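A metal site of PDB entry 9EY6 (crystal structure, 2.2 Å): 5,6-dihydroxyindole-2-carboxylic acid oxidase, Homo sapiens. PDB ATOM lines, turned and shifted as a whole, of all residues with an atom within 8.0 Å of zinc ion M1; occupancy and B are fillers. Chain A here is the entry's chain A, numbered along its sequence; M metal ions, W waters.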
ATOM      1  N   HIS A 168     -17.890   4.822 -22.882  1.00  0.00           N
ATOM      2  CA  HIS A 168     -19.037   5.549 -22.345  1.00  0.00           C
ATOM      3  C   HIS A 168     -20.292   5.256 -23.188  1.00  0.00           C
ATOM      4  O   HIS A 168     -21.358   5.015 -22.627  1.00  0.00           O
ATOM      5  CB  HIS A 168     -18.746   7.057 -22.245  1.00  0.00           C
ATOM      6  CG  HIS A 168     -19.721   7.911 -21.456  1.00  0.00           C
ATOM      7  ND1 HIS A 168     -20.832   8.491 -22.022  1.00  0.00           N
ATOM      8  CD2 HIS A 168     -19.724   8.338 -20.157  1.00  0.00           C
ATOM      9  CE1 HIS A 168     -21.448   9.262 -21.111  1.00  0.00           C
ATOM     10  NE2 HIS A 168     -20.827   9.151 -19.934  1.00  0.00           N
ATOM     11  N   TYR A 169     -20.159   5.251 -24.509  1.00  0.00           N
ATOM     12  CA  TYR A 169     -21.246   4.923 -25.418  1.00  0.00           C
ATOM     13  C   TYR A 169     -21.789   3.518 -25.132  1.00  0.00           C
ATOM     14  O   TYR A 169     -22.997   3.343 -24.982  1.00  0.00           O
ATOM     15  CB  TYR A 169     -20.769   5.045 -26.880  1.00  0.00           C
ATOM     16  CG  TYR A 169     -21.477   4.091 -27.836  1.00  0.00           C
ATOM     17  CD1 TYR A 169     -22.736   4.359 -28.359  1.00  0.00           C
ATOM     18  CD2 TYR A 169     -20.870   2.909 -28.202  1.00  0.00           C
ATOM     19  CE1 TYR A 169     -23.396   3.451 -29.182  1.00  0.00           C
ATOM     20  CE2 TYR A 169     -21.511   1.978 -28.995  1.00  0.00           C
ATOM     21  CZ  TYR A 169     -22.774   2.242 -29.494  1.00  0.00           C
ATOM     22  OH  TYR A 169     -23.289   1.267 -30.312  1.00  0.00           O
ATOM     23  N   SER A 171     -21.659   1.716 -22.538  1.00  0.00           N
ATOM     24  CA  SER A 171     -22.345   1.635 -21.256  1.00  0.00           C
ATOM     25  C   SER A 171     -23.776   2.174 -21.258  1.00  0.00           C
ATOM     26  O   SER A 171     -24.525   1.877 -20.306  1.00  0.00           O
ATOM     27  CB  SER A 171     -21.516   2.303 -20.163  1.00  0.00           C
ATOM     28  OG  SER A 171     -21.578   3.716 -20.187  1.00  0.00           O
ATOM     29  N   VAL A 172     -24.164   2.999 -22.259  1.00  0.00           N
ATOM     30  CA  VAL A 172     -25.469   3.652 -22.280  1.00  0.00           C
ATOM     31  C   VAL A 172     -26.324   3.192 -23.458  1.00  0.00           C
ATOM     32  O   VAL A 172     -27.480   3.559 -23.546  1.00  0.00           O
ATOM     33  CB  VAL A 172     -25.437   5.208 -22.234  1.00  0.00           C
ATOM     34  CG1 VAL A 172     -24.638   5.758 -21.066  1.00  0.00           C
ATOM     35  CG2 VAL A 172     -24.948   5.839 -23.530  1.00  0.00           C
ATOM     36  N   ASP A 188     -28.980   1.719 -18.192  1.00  0.00           N
ATOM     37  CA  ASP A 188     -27.813   2.578 -18.237  1.00  0.00           C
ATOM     38  C   ASP A 188     -26.802   2.069 -17.207  1.00  0.00           C
ATOM     39  O   ASP A 188     -27.015   2.232 -16.009  1.00  0.00           O
ATOM     40  CB  ASP A 188     -28.221   4.019 -17.975  1.00  0.00           C
ATOM     41  CG  ASP A 188     -27.185   5.101 -18.298  1.00  0.00           C
ATOM     42  OD1 ASP A 188     -25.977   4.882 -17.979  1.00  0.00           O
ATOM     43  OD2 ASP A 188     -27.591   6.183 -18.839  1.00  0.00           O
ATOM     44  N   SER A 190     -23.948   3.231 -16.294  1.00  0.00           N
ATOM     45  CA  SER A 190     -22.993   4.227 -15.803  1.00  0.00           C
ATOM     46  C   SER A 190     -23.682   5.490 -15.285  1.00  0.00           C
ATOM     47  O   SER A 190     -23.013   6.355 -14.740  1.00  0.00           O
ATOM     48  CB  SER A 190     -22.024   4.584 -16.847  1.00  0.00           C
ATOM     49  OG  SER A 190     -22.666   4.824 -18.106  1.00  0.00           O
ATOM     50  N   HIS A 191     -25.010   5.606 -15.432  1.00  0.00           N
ATOM     51  CA  HIS A 191     -25.754   6.751 -14.925  1.00  0.00           C
ATOM     52  C   HIS A 191     -27.045   6.250 -14.274  1.00  0.00           C
ATOM     53  O   HIS A 191     -27.466   5.113 -14.519  1.00  0.00           O
ATOM     54  CB  HIS A 191     -26.105   7.713 -16.076  1.00  0.00           C
ATOM     55  CG  HIS A 191     -24.951   8.060 -16.974  1.00  0.00           C
ATOM     56  ND1 HIS A 191     -24.535   7.227 -17.989  1.00  0.00           N
ATOM     57  CD2 HIS A 191     -24.099   9.085 -16.963  1.00  0.00           C
ATOM     58  CE1 HIS A 191     -23.462   7.749 -18.556  1.00  0.00           C
ATOM     59  NE2 HIS A 191     -23.208   8.901 -17.971  1.00  0.00           N
ATOM     60  N   PHE A 196     -22.773   5.530 -10.816  1.00  0.00           N
ATOM     61  CA  PHE A 196     -22.421   6.752 -11.545  1.00  0.00           C
ATOM     62  C   PHE A 196     -20.985   7.242 -11.244  1.00  0.00           C
ATOM     63  O   PHE A 196     -20.171   7.392 -12.174  1.00  0.00           O
ATOM     64  CB  PHE A 196     -23.443   7.854 -11.292  1.00  0.00           C
ATOM     65  CG  PHE A 196     -23.028   9.235 -11.761  1.00  0.00           C
ATOM     66  CD1 PHE A 196     -22.873   9.513 -13.102  1.00  0.00           C
ATOM     67  CD2 PHE A 196     -22.732  10.222 -10.848  1.00  0.00           C
ATOM     68  CE1 PHE A 196     -22.456  10.765 -13.508  1.00  0.00           C
ATOM     69  CE2 PHE A 196     -22.320  11.467 -11.261  1.00  0.00           C
ATOM     70  CZ  PHE A 196     -22.185  11.749 -12.592  1.00  0.00           C
ATOM     71  N   TRP A 199     -18.040   4.451 -11.680  1.00  0.00           N
ATOM     72  CA  TRP A 199     -17.829   4.230 -13.114  1.00  0.00           C
ATOM     73  C   TRP A 199     -16.989   5.358 -13.719  1.00  0.00           C
ATOM     74  O   TRP A 199     -15.963   5.113 -14.367  1.00  0.00           O
ATOM     75  CB  TRP A 199     -19.159   4.039 -13.852  1.00  0.00           C
ATOM     76  CG  TRP A 199     -19.028   3.508 -15.259  1.00  0.00           C
ATOM     77  CD1 TRP A 199     -19.265   2.234 -15.648  1.00  0.00           C
ATOM     78  CD2 TRP A 199     -18.610   4.200 -16.456  1.00  0.00           C
ATOM     79  NE1 TRP A 199     -18.990   2.078 -16.985  1.00  0.00           N
ATOM     80  CE2 TRP A 199     -18.577   3.265 -17.498  1.00  0.00           C
ATOM     81  CE3 TRP A 199     -18.217   5.512 -16.729  1.00  0.00           C
ATOM     82  CZ2 TRP A 199     -18.216   3.577 -18.791  1.00  0.00           C
ATOM     83  CZ3 TRP A 199     -17.879   5.844 -18.028  1.00  0.00           C
ATOM     84  CH2 TRP A 199     -17.860   4.896 -19.028  1.00  0.00           C
ATOM     85  N   HIS A 200     -17.388   6.612 -13.501  1.00  0.00           N
ATOM     86  CA  HIS A 200     -16.714   7.750 -14.132  1.00  0.00           C
ATOM     87  C   HIS A 200     -15.326   7.951 -13.549  1.00  0.00           C
ATOM     88  O   HIS A 200     -14.430   8.453 -14.201  1.00  0.00           O
ATOM     89  CB  HIS A 200     -17.595   9.014 -14.048  1.00  0.00           C
ATOM     90  CG  HIS A 200     -18.775   8.995 -14.974  1.00  0.00           C
ATOM     91  ND1 HIS A 200     -19.921   8.291 -14.668  1.00  0.00           N
ATOM     92  CD2 HIS A 200     -18.988   9.550 -16.214  1.00  0.00           C
ATOM     93  CE1 HIS A 200     -20.795   8.431 -15.678  1.00  0.00           C
ATOM     94  NE2 HIS A 200     -20.269   9.195 -16.631  1.00  0.00           N
ATOM     95  N   HIS A 203     -13.123   5.467 -15.451  1.00  0.00           N
ATOM     96  CA  HIS A 203     -13.048   6.012 -16.803  1.00  0.00           C
ATOM     97  C   HIS A 203     -11.885   7.002 -16.927  1.00  0.00           C
ATOM     98  O   HIS A 203     -11.097   6.884 -17.853  1.00  0.00           O
ATOM     99  CB  HIS A 203     -14.385   6.706 -17.068  1.00  0.00           C
ATOM    100  CG  HIS A 203     -14.653   7.018 -18.461  1.00  0.00           C
ATOM    101  ND1 HIS A 203     -15.339   8.168 -18.827  1.00  0.00           N
ATOM    102  CD2 HIS A 203     -14.400   6.335 -19.598  1.00  0.00           C
ATOM    103  CE1 HIS A 203     -15.483   8.159 -20.145  1.00  0.00           C
ATOM    104  NE2 HIS A 203     -14.901   7.057 -20.651  1.00  0.00           N
ATOM    105  N   GLU A 336     -25.051  13.838  -8.999  1.00  0.00           N
ATOM    106  CA  GLU A 336     -25.326  13.520 -10.389  1.00  0.00           C
ATOM    107  C   GLU A 336     -26.187  14.645 -10.970  1.00  0.00           C
ATOM    108  O   GLU A 336     -26.112  14.928 -12.175  1.00  0.00           O
ATOM    109  CB  GLU A 336     -25.923  12.118 -10.523  1.00  0.00           C
ATOM    110  CG  GLU A 336     -26.142  11.654 -11.973  1.00  0.00           C
ATOM    111  CD  GLU A 336     -26.526  10.180 -12.178  1.00  0.00           C
ATOM    112  OE1 GLU A 336     -26.720   9.473 -11.159  1.00  0.00           O
ATOM    113  OE2 GLU A 336     -26.674   9.710 -13.352  1.00  0.00           O
ATOM    114  N   HIS A 353     -23.754  18.097 -11.770  1.00  0.00           N
ATOM    115  CA  HIS A 353     -23.129  17.479 -12.931  1.00  0.00           C
ATOM    116  C   HIS A 353     -24.013  17.609 -14.158  1.00  0.00           C
ATOM    117  O   HIS A 353     -23.528  17.919 -15.236  1.00  0.00           O
ATOM    118  CB  HIS A 353     -22.639  16.064 -12.592  1.00  0.00           C
ATOM    119  CG  HIS A 353     -22.755  15.097 -13.708  1.00  0.00           C
ATOM    120  ND1 HIS A 353     -23.901  14.437 -14.108  1.00  0.00           N
ATOM    121  CD2 HIS A 353     -21.769  14.739 -14.568  1.00  0.00           C
ATOM    122  CE1 HIS A 353     -23.595  13.711 -15.200  1.00  0.00           C
ATOM    123  NE2 HIS A 353     -22.285  13.875 -15.479  1.00  0.00           N
ATOM    124  N   ASN A 354     -25.313  17.319 -14.012  1.00  0.00           N
ATOM    125  CA  ASN A 354     -26.222  17.323 -15.160  1.00  0.00           C
ATOM    126  C   ASN A 354     -26.391  18.754 -15.701  1.00  0.00           C
ATOM    127  O   ASN A 354     -26.529  18.932 -16.900  1.00  0.00           O
ATOM    128  CB  ASN A 354     -27.587  16.729 -14.855  1.00  0.00           C
ATOM    129  CG  ASN A 354     -27.610  15.223 -14.662  1.00  0.00           C
ATOM    130  OD1 ASN A 354     -26.832  14.456 -15.257  1.00  0.00           O
ATOM    131  ND2 ASN A 354     -28.543  14.790 -13.843  1.00  0.00           N
ATOM    132  N   HIS A 357     -23.337  19.719 -17.875  1.00  0.00           N
ATOM    133  CA  HIS A 357     -23.484  19.191 -19.220  1.00  0.00           C
ATOM    134  C   HIS A 357     -24.495  19.990 -20.043  1.00  0.00           C
ATOM    135  O   HIS A 357     -24.289  20.275 -21.227  1.00  0.00           O
ATOM    136  CB  HIS A 357     -23.965  17.734 -19.173  1.00  0.00           C
ATOM    137  CG  HIS A 357     -22.960  16.659 -18.956  1.00  0.00           C
ATOM    138  ND1 HIS A 357     -22.169  16.176 -19.986  1.00  0.00           N
ATOM    139  CD2 HIS A 357     -22.623  15.949 -17.881  1.00  0.00           C
ATOM    140  CE1 HIS A 357     -21.393  15.202 -19.534  1.00  0.00           C
ATOM    141  NE2 HIS A 357     -21.661  15.024 -18.276  1.00  0.00           N
ATOM    142  N   GLN A 366     -25.473  15.359 -24.912  1.00  0.00           N
ATOM    143  CA  GLN A 366     -26.181  14.172 -25.363  1.00  0.00           C
ATOM    144  C   GLN A 366     -25.432  12.926 -24.865  1.00  0.00           C
ATOM    145  O   GLN A 366     -24.228  12.782 -25.102  1.00  0.00           O
ATOM    146  CB  GLN A 366     -26.209  14.271 -26.888  1.00  0.00           C
ATOM    147  CG  GLN A 366     -26.698  15.628 -27.398  1.00  0.00           C
ATOM    148  CD  GLN A 366     -26.549  15.788 -28.886  1.00  0.00           C
ATOM    149  OE1 GLN A 366     -27.123  15.041 -29.687  1.00  0.00           O
ATOM    150  NE2 GLN A 366     -25.782  16.798 -29.287  1.00  0.00           N
ATOM    151  N   THR A 367     -26.154  12.028 -24.189  1.00  0.00           N
ATOM    152  CA  THR A 367     -25.494  11.069 -23.299  1.00  0.00           C
ATOM    153  C   THR A 367     -24.628  10.099 -24.095  1.00  0.00           C
ATOM    154  O   THR A 367     -23.502   9.810 -23.670  1.00  0.00           O
ATOM    155  CB  THR A 367     -26.456  10.354 -22.353  1.00  0.00           C
ATOM    156  OG1 THR A 367     -27.243  11.356 -21.702  1.00  0.00           O
ATOM    157  CG2 THR A 367     -25.694   9.575 -21.289  1.00  0.00           C
ATOM    158  N   HIS A 368     -25.068   9.701 -25.309  1.00  0.00           N
ATOM    159  CA  HIS A 368     -24.240   8.816 -26.124  1.00  0.00           C
ATOM    160  C   HIS A 368     -23.023   9.490 -26.786  1.00  0.00           C
ATOM    161  O   HIS A 368     -22.127   8.767 -27.248  1.00  0.00           O
ATOM    162  CB  HIS A 368     -25.050   8.098 -27.208  1.00  0.00           C
ATOM    163  CG  HIS A 368     -25.617   9.036 -28.210  1.00  0.00           C
ATOM    164  ND1 HIS A 368     -26.505  10.018 -27.815  1.00  0.00           N
ATOM    165  CD2 HIS A 368     -25.413   9.201 -29.524  1.00  0.00           C
ATOM    166  CE1 HIS A 368     -26.839  10.748 -28.882  1.00  0.00           C
ATOM    167  NE2 HIS A 368     -26.192  10.269 -29.931  1.00  0.00           N
ATOM    168  N   SER A 370     -21.348  12.591 -25.269  1.00  0.00           N
ATOM    169  CA  SER A 370     -20.822  13.734 -24.535  1.00  0.00           C
ATOM    170  C   SER A 370     -19.296  13.754 -24.417  1.00  0.00           C
ATOM    171  O   SER A 370     -18.724  14.833 -24.349  1.00  0.00           O
ATOM    172  CB  SER A 370     -21.475  13.918 -23.176  1.00  0.00           C
ATOM    173  OG  SER A 370     -21.606  12.700 -22.494  1.00  0.00           O
ATOM    174  N   PRO A 371     -18.590  12.615 -24.247  1.00  0.00           N
ATOM    175  CA  PRO A 371     -17.132  12.657 -24.122  1.00  0.00           C
ATOM    176  C   PRO A 371     -16.407  13.124 -25.368  1.00  0.00           C
ATOM    177  O   PRO A 371     -15.236  13.463 -25.259  1.00  0.00           O
ATOM    178  CB  PRO A 371     -16.711  11.236 -23.725  1.00  0.00           C
ATOM    179  CG  PRO A 371     -17.991  10.510 -23.448  1.00  0.00           C
ATOM    180  CD  PRO A 371     -19.120  11.249 -24.099  1.00  0.00           C
ATOM    181  N   PHE A 376     -15.776  17.398 -21.170  1.00  0.00           N
ATOM    182  CA  PHE A 376     -16.190  16.214 -20.440  1.00  0.00           C
ATOM    183  C   PHE A 376     -15.106  15.780 -19.448  1.00  0.00           C
ATOM    184  O   PHE A 376     -15.413  15.534 -18.303  1.00  0.00           O
ATOM    185  CB  PHE A 376     -16.513  15.066 -21.401  1.00  0.00           C
ATOM    186  CG  PHE A 376     -17.011  13.788 -20.719  1.00  0.00           C
ATOM    187  CD1 PHE A 376     -16.126  12.907 -20.133  1.00  0.00           C
ATOM    188  CD2 PHE A 376     -18.360  13.449 -20.736  1.00  0.00           C
ATOM    189  CE1 PHE A 376     -16.582  11.755 -19.527  1.00  0.00           C
ATOM    190  CE2 PHE A 376     -18.835  12.288 -20.122  1.00  0.00           C
ATOM    191  CZ  PHE A 376     -17.939  11.430 -19.534  1.00  0.00           C
ATOM    192  N   HIS A 380     -15.814  15.948 -15.437  1.00  0.00           N
ATOM    193  CA  HIS A 380     -15.776  14.699 -14.673  1.00  0.00           C
ATOM    194  C   HIS A 380     -14.664  14.669 -13.624  1.00  0.00           C
ATOM    195  O   HIS A 380     -14.872  14.044 -12.589  1.00  0.00           O
ATOM    196  CB  HIS A 380     -15.871  13.459 -15.592  1.00  0.00           C
ATOM    197  CG  HIS A 380     -17.307  13.156 -15.837  1.00  0.00           C
ATOM    198  ND1 HIS A 380     -18.022  12.593 -14.791  1.00  0.00           N
ATOM    199  CD2 HIS A 380     -18.200  13.434 -16.823  1.00  0.00           C
ATOM    200  CE1 HIS A 380     -19.296  12.511 -15.156  1.00  0.00           C
ATOM    201  NE2 HIS A 380     -19.426  13.014 -16.380  1.00  0.00           N
HETATM  202 ZN    ZN M   1     -21.413   9.898 -18.225  1.00  0.00          ZN
HETATM  203 ZN    ZN M   2     -21.225  13.336 -17.147  1.00  0.00          ZN
HETATM  204  O   HOH W   1     -21.701  12.111 -18.109  1.00  0.00           O
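Zinc ion M1 is bound by a ring nitrogen (NE2) of His 168 (2.0 Å), a ring nitrogen (NE2) of His 191 (2.1 Å), a ring nitrogen (NE2) of His 200 (2.1 Å) and water W1 (2.2 Å).
A ring nitrogen (ND1) of His 168 sits close to the backbone carbonyl oxygen of Thr 367. A ring nitrogen (ND1) of His 191 lies within hydrogen-bond range of the side-chain hydroxyl (OG) of Ser 190, 3.0 Å away. A ring nitrogen (ND1) of His 191 sits at hydrogen-bond distance from the side-chain carboxylate of Asp 188 (2.8 Å). O of His 168 lies within hydrogen-bond range of OG of Ser 171 (2.8 Å). The backbone carbonyl oxygen (O) of Phe 196 lies within hydrogen-bond range of a ring nitrogen (ND1) of His 200, at 2.7 Å.
Merely in contact with zinc ion M1: Phe 376. Within 4 Å of zinc ion M1: His 168, His 191, His 200 and Phe 376. Along chain A the residues within 4 Å of zinc ion M1 span positions 168 to 376.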
